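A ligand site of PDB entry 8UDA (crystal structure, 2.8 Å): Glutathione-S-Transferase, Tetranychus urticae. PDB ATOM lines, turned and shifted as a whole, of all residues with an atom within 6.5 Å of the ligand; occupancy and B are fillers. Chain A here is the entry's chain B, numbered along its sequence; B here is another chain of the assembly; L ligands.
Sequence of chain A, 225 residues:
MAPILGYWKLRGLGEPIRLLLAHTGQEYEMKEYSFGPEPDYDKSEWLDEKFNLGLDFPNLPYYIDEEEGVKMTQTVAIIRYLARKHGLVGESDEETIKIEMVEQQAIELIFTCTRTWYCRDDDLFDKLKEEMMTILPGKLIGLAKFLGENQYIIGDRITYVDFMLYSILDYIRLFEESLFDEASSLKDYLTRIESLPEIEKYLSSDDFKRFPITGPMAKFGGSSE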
ATOM      1  N   TYR A   7     -20.054 -10.020 -35.667  1.00  0.00           N
ATOM      2  CA  TYR A   7     -18.814  -9.410 -35.211  1.00  0.00           C
ATOM      3  C   TYR A   7     -18.452  -8.244 -36.128  1.00  0.00           C
ATOM      4  O   TYR A   7     -19.121  -8.010 -37.122  1.00  0.00           O
ATOM      5  CB  TYR A   7     -17.657 -10.432 -35.197  1.00  0.00           C
ATOM      6  CG  TYR A   7     -16.409  -9.961 -34.498  1.00  0.00           C
ATOM      7  CD1 TYR A   7     -16.448  -9.572 -33.169  1.00  0.00           C
ATOM      8  CD2 TYR A   7     -15.189  -9.890 -35.158  1.00  0.00           C
ATOM      9  CE1 TYR A   7     -15.313  -9.114 -32.517  1.00  0.00           C
ATOM     10  CE2 TYR A   7     -14.046  -9.432 -34.518  1.00  0.00           C
ATOM     11  CZ  TYR A   7     -14.104  -9.053 -33.194  1.00  0.00           C
ATOM     12  OH  TYR A   7     -13.038  -8.592 -32.461  1.00  0.00           O
ATOM     13  N   TRP A   8     -17.382  -7.518 -35.806  1.00  0.00           N
ATOM     14  CA  TRP A   8     -16.890  -6.444 -36.638  1.00  0.00           C
ATOM     15  C   TRP A   8     -16.238  -6.989 -37.909  1.00  0.00           C
ATOM     16  O   TRP A   8     -15.989  -8.194 -38.008  1.00  0.00           O
ATOM     17  CB  TRP A   8     -15.870  -5.631 -35.839  1.00  0.00           C
ATOM     18  CG  TRP A   8     -16.454  -4.943 -34.650  1.00  0.00           C
ATOM     19  CD1 TRP A   8     -16.216  -5.251 -33.336  1.00  0.00           C
ATOM     20  CD2 TRP A   8     -17.344  -3.810 -34.659  1.00  0.00           C
ATOM     21  NE1 TRP A   8     -16.913  -4.385 -32.524  1.00  0.00           N
ATOM     22  CE2 TRP A   8     -17.601  -3.493 -33.302  1.00  0.00           C
ATOM     23  CE3 TRP A   8     -17.947  -3.055 -35.674  1.00  0.00           C
ATOM     24  CZ2 TRP A   8     -18.424  -2.422 -32.941  1.00  0.00           C
ATOM     25  CZ3 TRP A   8     -18.769  -2.001 -35.328  1.00  0.00           C
ATOM     26  CH2 TRP A   8     -18.998  -1.708 -33.975  1.00  0.00           C
ATOM     27  N   LEU A  10     -13.291  -6.665 -38.612  1.00  0.00           N
ATOM     28  CA  LEU A  10     -11.914  -6.977 -38.287  1.00  0.00           C
ATOM     29  C   LEU A  10     -11.811  -8.462 -37.965  1.00  0.00           C
ATOM     30  O   LEU A  10     -12.837  -9.126 -37.853  1.00  0.00           O
ATOM     31  CB  LEU A  10     -11.521  -6.154 -37.070  1.00  0.00           C
ATOM     32  CG  LEU A  10     -12.280  -4.839 -36.915  1.00  0.00           C
ATOM     33  CD1 LEU A  10     -12.267  -4.390 -35.464  1.00  0.00           C
ATOM     34  CD2 LEU A  10     -11.747  -3.764 -37.858  1.00  0.00           C
ATOM     35  N   GLY A  12      -9.725  -9.928 -35.209  1.00  0.00           N
ATOM     36  CA  GLY A  12      -9.927  -9.810 -33.772  1.00  0.00           C
ATOM     37  C   GLY A  12     -10.333 -11.121 -33.107  1.00  0.00           C
ATOM     38  O   GLY A  12      -9.681 -12.134 -33.344  1.00  0.00           O
ATOM     39  N   LEU A  13     -11.432 -11.088 -32.337  1.00  0.00           N
ATOM     40  CA  LEU A  13     -11.874 -12.207 -31.526  1.00  0.00           C
ATOM     41  C   LEU A  13     -12.682 -13.191 -32.370  1.00  0.00           C
ATOM     42  O   LEU A  13     -12.814 -14.340 -31.988  1.00  0.00           O
ATOM     43  CB  LEU A  13     -12.755 -11.698 -30.379  1.00  0.00           C
ATOM     44  CG  LEU A  13     -12.188 -10.548 -29.540  1.00  0.00           C
ATOM     45  CD1 LEU A  13     -13.134 -10.130 -28.426  1.00  0.00           C
ATOM     46  CD2 LEU A  13     -10.853 -10.969 -28.966  1.00  0.00           C
ATOM     47  N   PHE A  35     -17.402   0.417 -38.937  1.00  0.00           N
ATOM     48  CA  PHE A  35     -17.322   1.626 -38.154  1.00  0.00           C
ATOM     49  C   PHE A  35     -17.694   2.833 -39.008  1.00  0.00           C
ATOM     50  O   PHE A  35     -17.955   2.692 -40.205  1.00  0.00           O
ATOM     51  CB  PHE A  35     -15.934   1.774 -37.541  1.00  0.00           C
ATOM     52  CG  PHE A  35     -15.549   0.675 -36.579  1.00  0.00           C
ATOM     53  CD1 PHE A  35     -15.231  -0.589 -37.028  1.00  0.00           C
ATOM     54  CD2 PHE A  35     -15.537   0.917 -35.211  1.00  0.00           C
ATOM     55  CE1 PHE A  35     -14.880  -1.588 -36.132  1.00  0.00           C
ATOM     56  CE2 PHE A  35     -15.166  -0.073 -34.309  1.00  0.00           C
ATOM     57  CZ  PHE A  35     -14.855  -1.323 -34.774  1.00  0.00           C
ATOM     58  N   LYS A  43     -19.522   3.290 -33.661  1.00  0.00           N
ATOM     59  CA  LYS A  43     -20.000   1.910 -33.618  1.00  0.00           C
ATOM     60  C   LYS A  43     -21.514   1.877 -33.820  1.00  0.00           C
ATOM     61  O   LYS A  43     -22.168   0.868 -33.544  1.00  0.00           O
ATOM     62  CB  LYS A  43     -19.555   1.267 -32.296  1.00  0.00           C
ATOM     63  CG  LYS A  43     -18.052   1.281 -32.075  1.00  0.00           C
ATOM     64  CD  LYS A  43     -17.658   0.663 -30.757  1.00  0.00           C
ATOM     65  CE  LYS A  43     -16.167   0.702 -30.511  1.00  0.00           C
ATOM     66  NZ  LYS A  43     -15.809   0.143 -29.180  1.00  0.00           N
ATOM     67  N   TRP A  46     -23.574  -1.086 -35.022  1.00  0.00           N
ATOM     68  CA  TRP A  46     -23.744  -2.101 -33.999  1.00  0.00           C
ATOM     69  C   TRP A  46     -24.749  -1.634 -32.941  1.00  0.00           C
ATOM     70  O   TRP A  46     -25.700  -2.351 -32.603  1.00  0.00           O
ATOM     71  CB  TRP A  46     -22.385  -2.466 -33.384  1.00  0.00           C
ATOM     72  CG  TRP A  46     -22.416  -3.199 -32.075  1.00  0.00           C
ATOM     73  CD1 TRP A  46     -21.739  -2.859 -30.943  1.00  0.00           C
ATOM     74  CD2 TRP A  46     -23.157  -4.398 -31.771  1.00  0.00           C
ATOM     75  NE1 TRP A  46     -22.027  -3.747 -29.945  1.00  0.00           N
ATOM     76  CE2 TRP A  46     -22.878  -4.710 -30.416  1.00  0.00           C
ATOM     77  CE3 TRP A  46     -24.018  -5.227 -32.495  1.00  0.00           C
ATOM     78  CZ2 TRP A  46     -23.431  -5.828 -29.777  1.00  0.00           C
ATOM     79  CZ3 TRP A  46     -24.565  -6.332 -31.860  1.00  0.00           C
ATOM     80  CH2 TRP A  46     -24.292  -6.627 -30.512  1.00  0.00           C
ATOM     81  N   LYS A  50     -27.849  -3.348 -31.055  1.00  0.00           N
ATOM     82  CA  LYS A  50     -27.158  -4.002 -29.938  1.00  0.00           C
ATOM     83  C   LYS A  50     -28.105  -4.672 -28.931  1.00  0.00           C
ATOM     84  O   LYS A  50     -27.972  -5.875 -28.632  1.00  0.00           O
ATOM     85  CB  LYS A  50     -26.234  -2.986 -29.258  1.00  0.00           C
ATOM     86  CG  LYS A  50     -25.490  -3.534 -28.047  1.00  0.00           C
ATOM     87  CD  LYS A  50     -24.399  -2.649 -27.508  1.00  0.00           C
ATOM     88  CE  LYS A  50     -23.793  -3.299 -26.287  1.00  0.00           C
ATOM     89  NZ  LYS A  50     -22.621  -2.548 -25.802  1.00  0.00           N
ATOM     90  N   PRO A  58     -25.235  -8.416 -24.436  1.00  0.00           N
ATOM     91  CA  PRO A  58     -25.038  -7.917 -25.793  1.00  0.00           C
ATOM     92  C   PRO A  58     -23.597  -7.457 -25.937  1.00  0.00           C
ATOM     93  O   PRO A  58     -23.099  -6.649 -25.144  1.00  0.00           O
ATOM     94  CB  PRO A  58     -26.038  -6.752 -25.921  1.00  0.00           C
ATOM     95  CG  PRO A  58     -26.327  -6.376 -24.486  1.00  0.00           C
ATOM     96  CD  PRO A  58     -26.301  -7.677 -23.731  1.00  0.00           C
ATOM     97  N   ASN A  59     -22.931  -8.027 -26.931  1.00  0.00           N
ATOM     98  CA  ASN A  59     -21.514  -7.810 -27.174  1.00  0.00           C
ATOM     99  C   ASN A  59     -21.188  -8.454 -28.512  1.00  0.00           C
ATOM    100  O   ASN A  59     -22.002  -9.218 -29.030  1.00  0.00           O
ATOM    101  CB  ASN A  59     -20.679  -8.465 -26.082  1.00  0.00           C
ATOM    102  CG  ASN A  59     -19.323  -7.828 -25.940  1.00  0.00           C
ATOM    103  OD1 ASN A  59     -18.937  -7.002 -26.763  1.00  0.00           O
ATOM    104  ND2 ASN A  59     -18.600  -8.219 -24.904  1.00  0.00           N
ATOM    105  N   LEU A  60     -20.033  -8.097 -29.081  1.00  0.00           N
ATOM    106  CA  LEU A  60     -19.505  -8.739 -30.270  1.00  0.00           C
ATOM    107  C   LEU A  60     -18.234  -9.516 -29.887  1.00  0.00           C
ATOM    108  O   LEU A  60     -17.341  -8.987 -29.225  1.00  0.00           O
ATOM    109  CB  LEU A  60     -19.229  -7.695 -31.357  1.00  0.00           C
ATOM    110  CG  LEU A  60     -20.478  -7.073 -31.994  1.00  0.00           C
ATOM    111  CD1 LEU A  60     -20.082  -5.993 -32.969  1.00  0.00           C
ATOM    112  CD2 LEU A  60     -21.324  -8.113 -32.695  1.00  0.00           C
ATOM    113  N   PRO A  61     -18.079 -10.778 -30.352  1.00  0.00           N
ATOM    114  CA  PRO A  61     -19.037 -11.383 -31.269  1.00  0.00           C
ATOM    115  C   PRO A  61     -20.264 -11.908 -30.522  1.00  0.00           C
ATOM    116  O   PRO A  61     -20.259 -11.994 -29.288  1.00  0.00           O
ATOM    117  CB  PRO A  61     -18.226 -12.547 -31.862  1.00  0.00           C
ATOM    118  CG  PRO A  61     -17.338 -12.970 -30.702  1.00  0.00           C
ATOM    119  CD  PRO A  61     -16.915 -11.648 -30.095  1.00  0.00           C
ATOM    120  N   PHE A 111      -5.042 -10.156 -23.812  1.00  0.00           N
ATOM    121  CA  PHE A 111      -5.069  -9.082 -22.817  1.00  0.00           C
ATOM    122  C   PHE A 111      -3.892  -8.118 -23.003  1.00  0.00           C
ATOM    123  O   PHE A 111      -4.076  -6.915 -23.243  1.00  0.00           O
ATOM    124  CB  PHE A 111      -5.079  -9.621 -21.389  1.00  0.00           C
ATOM    125  CG  PHE A 111      -4.679  -8.631 -20.312  1.00  0.00           C
ATOM    126  CD1 PHE A 111      -5.398  -7.453 -20.109  1.00  0.00           C
ATOM    127  CD2 PHE A 111      -3.580  -8.866 -19.492  1.00  0.00           C
ATOM    128  CE1 PHE A 111      -5.010  -6.534 -19.132  1.00  0.00           C
ATOM    129  CE2 PHE A 111      -3.201  -7.950 -18.513  1.00  0.00           C
ATOM    130  CZ  PHE A 111      -3.919  -6.788 -18.326  1.00  0.00           C
ATOM    131  N   THR A 114      -3.874  -6.299 -26.480  1.00  0.00           N
ATOM    132  CA  THR A 114      -4.927  -5.314 -26.653  1.00  0.00           C
ATOM    133  C   THR A 114      -4.614  -4.083 -25.796  1.00  0.00           C
ATOM    134  O   THR A 114      -4.648  -2.971 -26.307  1.00  0.00           O
ATOM    135  CB  THR A 114      -6.305  -5.902 -26.296  1.00  0.00           C
ATOM    136  OG1 THR A 114      -6.486  -6.999 -27.196  1.00  0.00           O
ATOM    137  CG2 THR A 114      -7.452  -4.906 -26.398  1.00  0.00           C
ATOM    138  N   ARG A 115      -4.277  -4.322 -24.518  1.00  0.00           N
ATOM    139  CA  ARG A 115      -3.954  -3.254 -23.590  1.00  0.00           C
ATOM    140  C   ARG A 115      -2.966  -2.282 -24.243  1.00  0.00           C
ATOM    141  O   ARG A 115      -3.017  -1.084 -23.979  1.00  0.00           O
ATOM    142  CB  ARG A 115      -3.437  -3.813 -22.265  1.00  0.00           C
ATOM    143  N   THR A 116      -2.092  -2.809 -25.104  1.00  0.00           N
ATOM    144  CA  THR A 116      -1.045  -2.022 -25.736  1.00  0.00           C
ATOM    145  C   THR A 116      -1.532  -1.418 -27.060  1.00  0.00           C
ATOM    146  O   THR A 116      -1.407  -0.219 -27.256  1.00  0.00           O
ATOM    147  CB  THR A 116       0.252  -2.813 -25.888  1.00  0.00           C
ATOM    148  OG1 THR A 116       0.671  -3.154 -24.570  1.00  0.00           O
ATOM    149  CG2 THR A 116       1.362  -2.037 -26.588  1.00  0.00           C
ATOM    150  N   TYR A 118      -4.248  -0.675 -28.157  1.00  0.00           N
ATOM    151  CA  TYR A 118      -5.353   0.272 -28.084  1.00  0.00           C
ATOM    152  C   TYR A 118      -4.961   1.564 -27.366  1.00  0.00           C
ATOM    153  O   TYR A 118      -5.671   2.546 -27.488  1.00  0.00           O
ATOM    154  CB  TYR A 118      -6.618  -0.377 -27.534  1.00  0.00           C
ATOM    155  CG  TYR A 118      -7.451  -1.073 -28.590  1.00  0.00           C
ATOM    156  CD1 TYR A 118      -7.044  -2.284 -29.145  1.00  0.00           C
ATOM    157  CD2 TYR A 118      -8.612  -0.490 -29.073  1.00  0.00           C
ATOM    158  CE1 TYR A 118      -7.801  -2.922 -30.113  1.00  0.00           C
ATOM    159  CE2 TYR A 118      -9.367  -1.111 -30.058  1.00  0.00           C
ATOM    160  CZ  TYR A 118      -8.958  -2.314 -30.594  1.00  0.00           C
ATOM    161  OH  TYR A 118      -9.699  -2.905 -31.571  1.00  0.00           O
ATOM    162  N   CYS A 119      -3.851   1.563 -26.625  1.00  0.00           N
ATOM    163  CA  CYS A 119      -3.326   2.786 -26.023  1.00  0.00           C
ATOM    164  C   CYS A 119      -2.877   3.725 -27.143  1.00  0.00           C
ATOM    165  O   CYS A 119      -2.203   3.308 -28.089  1.00  0.00           O
ATOM    166  CB  CYS A 119      -2.167   2.481 -25.076  1.00  0.00           C
ATOM    167  SG  CYS A 119      -1.527   3.919 -24.193  1.00  0.00           S
ATOM    168  N   THR A 214      -7.199  -5.250 -35.561  1.00  0.00           N
ATOM    169  CA  THR A 214      -7.891  -4.470 -34.546  1.00  0.00           C
ATOM    170  C   THR A 214      -8.764  -3.405 -35.208  1.00  0.00           C
ATOM    171  O   THR A 214      -8.794  -3.304 -36.434  1.00  0.00           O
ATOM    172  CB  THR A 214      -6.921  -3.769 -33.592  1.00  0.00           C
ATOM    173  OG1 THR A 214      -5.945  -3.142 -34.425  1.00  0.00           O
ATOM    174  CG2 THR A 214      -6.253  -4.702 -32.614  1.00  0.00           C
ATOM    175  N   GLY A 215      -9.505  -2.644 -34.395  1.00  0.00           N
ATOM    176  CA  GLY A 215     -10.332  -1.571 -34.882  1.00  0.00           C
ATOM    177  C   GLY A 215      -9.496  -0.473 -35.523  1.00  0.00           C
ATOM    178  O   GLY A 215      -8.300  -0.371 -35.270  1.00  0.00           O
ATOM    179  N   MET A 217      -9.558   2.366 -34.694  1.00  0.00           N
ATOM    180  CA  MET A 217      -9.243   3.192 -33.546  1.00  0.00           C
ATOM    181  C   MET A 217      -7.855   2.849 -32.963  1.00  0.00           C
ATOM    182  O   MET A 217      -7.223   3.694 -32.339  1.00  0.00           O
ATOM    183  CB  MET A 217     -10.296   3.015 -32.455  1.00  0.00           C
ATOM    184  CG  MET A 217     -10.354   1.580 -31.974  1.00  0.00           C
ATOM    185  SD  MET A 217     -11.813   1.091 -31.066  1.00  0.00           S
ATOM    186  CE  MET A 217     -12.849   0.714 -32.479  1.00  0.00           C
ATOM    187  N   ARG B 115      -7.101  -2.798 -15.440  1.00  0.00           N
ATOM    188  CA  ARG B 115      -6.395  -1.796 -16.225  1.00  0.00           C
ATOM    189  C   ARG B 115      -6.521  -0.452 -15.514  1.00  0.00           C
ATOM    190  O   ARG B 115      -5.680   0.419 -15.705  1.00  0.00           O
ATOM    191  CB  ARG B 115      -6.914  -1.744 -17.660  1.00  0.00           C
ATOM    192  CG  ARG B 115      -8.370  -1.306 -17.788  1.00  0.00           C
ATOM    193  CD  ARG B 115      -8.749  -1.130 -19.241  1.00  0.00           C
ATOM    194  NE  ARG B 115     -10.185  -0.924 -19.446  1.00  0.00           N
ATOM    195  CZ  ARG B 115     -10.986  -1.736 -20.118  1.00  0.00           C
ATOM    196  NH1 ARG B 115     -10.584  -2.966 -20.429  1.00  0.00           N
ATOM    197  NH2 ARG B 115     -12.200  -1.334 -20.452  1.00  0.00           N
HETATM  198  N1  LIG L   1      -9.708  -0.540 -25.899  1.00  0.00           N
HETATM  199  C1  LIG L   1     -10.076  -1.613 -24.931  1.00  0.00           C
HETATM  200  C2  LIG L   1      -8.869  -1.887 -24.012  1.00  0.00           C
HETATM  201  O1  LIG L   1      -7.808  -2.207 -24.562  1.00  0.00           O
HETATM  202  O2  LIG L   1      -9.045  -1.732 -22.795  1.00  0.00           O
HETATM  203  C3  LIG L   1     -10.584  -2.852 -25.667  1.00  0.00           C
HETATM  204  C4  LIG L   1     -10.977  -2.542 -27.106  1.00  0.00           C
HETATM  205  C5  LIG L   1     -11.626  -3.605 -27.958  1.00  0.00           C
HETATM  206  O3  LIG L   1     -11.118  -4.707 -28.102  1.00  0.00           O
HETATM  207  N2  LIG L   1     -12.812  -3.217 -28.429  1.00  0.00           N
HETATM  208  C6  LIG L   1     -13.149  -3.029 -29.827  1.00  0.00           C
HETATM  209  C7  LIG L   1     -14.636  -2.827 -30.121  1.00  0.00           C
HETATM  210  O4  LIG L   1     -14.968  -2.403 -31.221  1.00  0.00           O
HETATM  211  C8  LIG L   1     -12.525  -4.064 -30.760  1.00  0.00           C
HETATM  212  S1  LIG L   1     -13.222  -5.730 -30.597  1.00  0.00           S
HETATM  213  N3  LIG L   1     -15.504  -3.094 -29.134  1.00  0.00           N
HETATM  214  C9  LIG L   1     -16.938  -3.126 -29.356  1.00  0.00           C
HETATM  215  C10 LIG L   1     -17.561  -4.482 -29.016  1.00  0.00           C
HETATM  216  O5  LIG L   1     -17.071  -5.477 -29.585  1.00  0.00           O
HETATM  217  O6  LIG L   1     -18.516  -4.503 -28.198  1.00  0.00           O
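Residues that only touch the ligand: Tyr 118 (3.2 Å), Thr 114 (3.3 Å), Leu 60 (3.5 Å), Phe 35 (3.7 Å), Met 217 (3.97 Å) and Trp 46 (3.99 Å).
Hydrophobic or aromatic side chains that line the ligand: Trp 8, Phe 35, Leu 60, Tyr 118 and Met 217.
The indole nitrogen (NE1) of Trp 8 is in hydrogen-bond range of an oxygen (O4) of the ligand.
The side-chain amide oxygen of Asn 59 sits close to an oxygen (O6) of the ligand (2.9 Å).
An oxygen (O2) of the ligand is in salt-bridge range of the guanidinium group of Arg 115 of chain B (3.1 Å).
The side-chain amino group (NZ) of Lys 43 sits close to an oxygen (O4) of the ligand (3.4 Å).
S1 of the ligand lies close to OH of Tyr 7 (3.4 Å).
The backbone NH (N) of Leu 13 is in hydrogen-bond range of the side-chain hydroxyl (OH) of Tyr 7 (3.0 Å).
The backbone NH of Gly 215 is in hydrogen-bond range of the side-chain hydroxyl of Tyr 118, 2.8 Å away.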
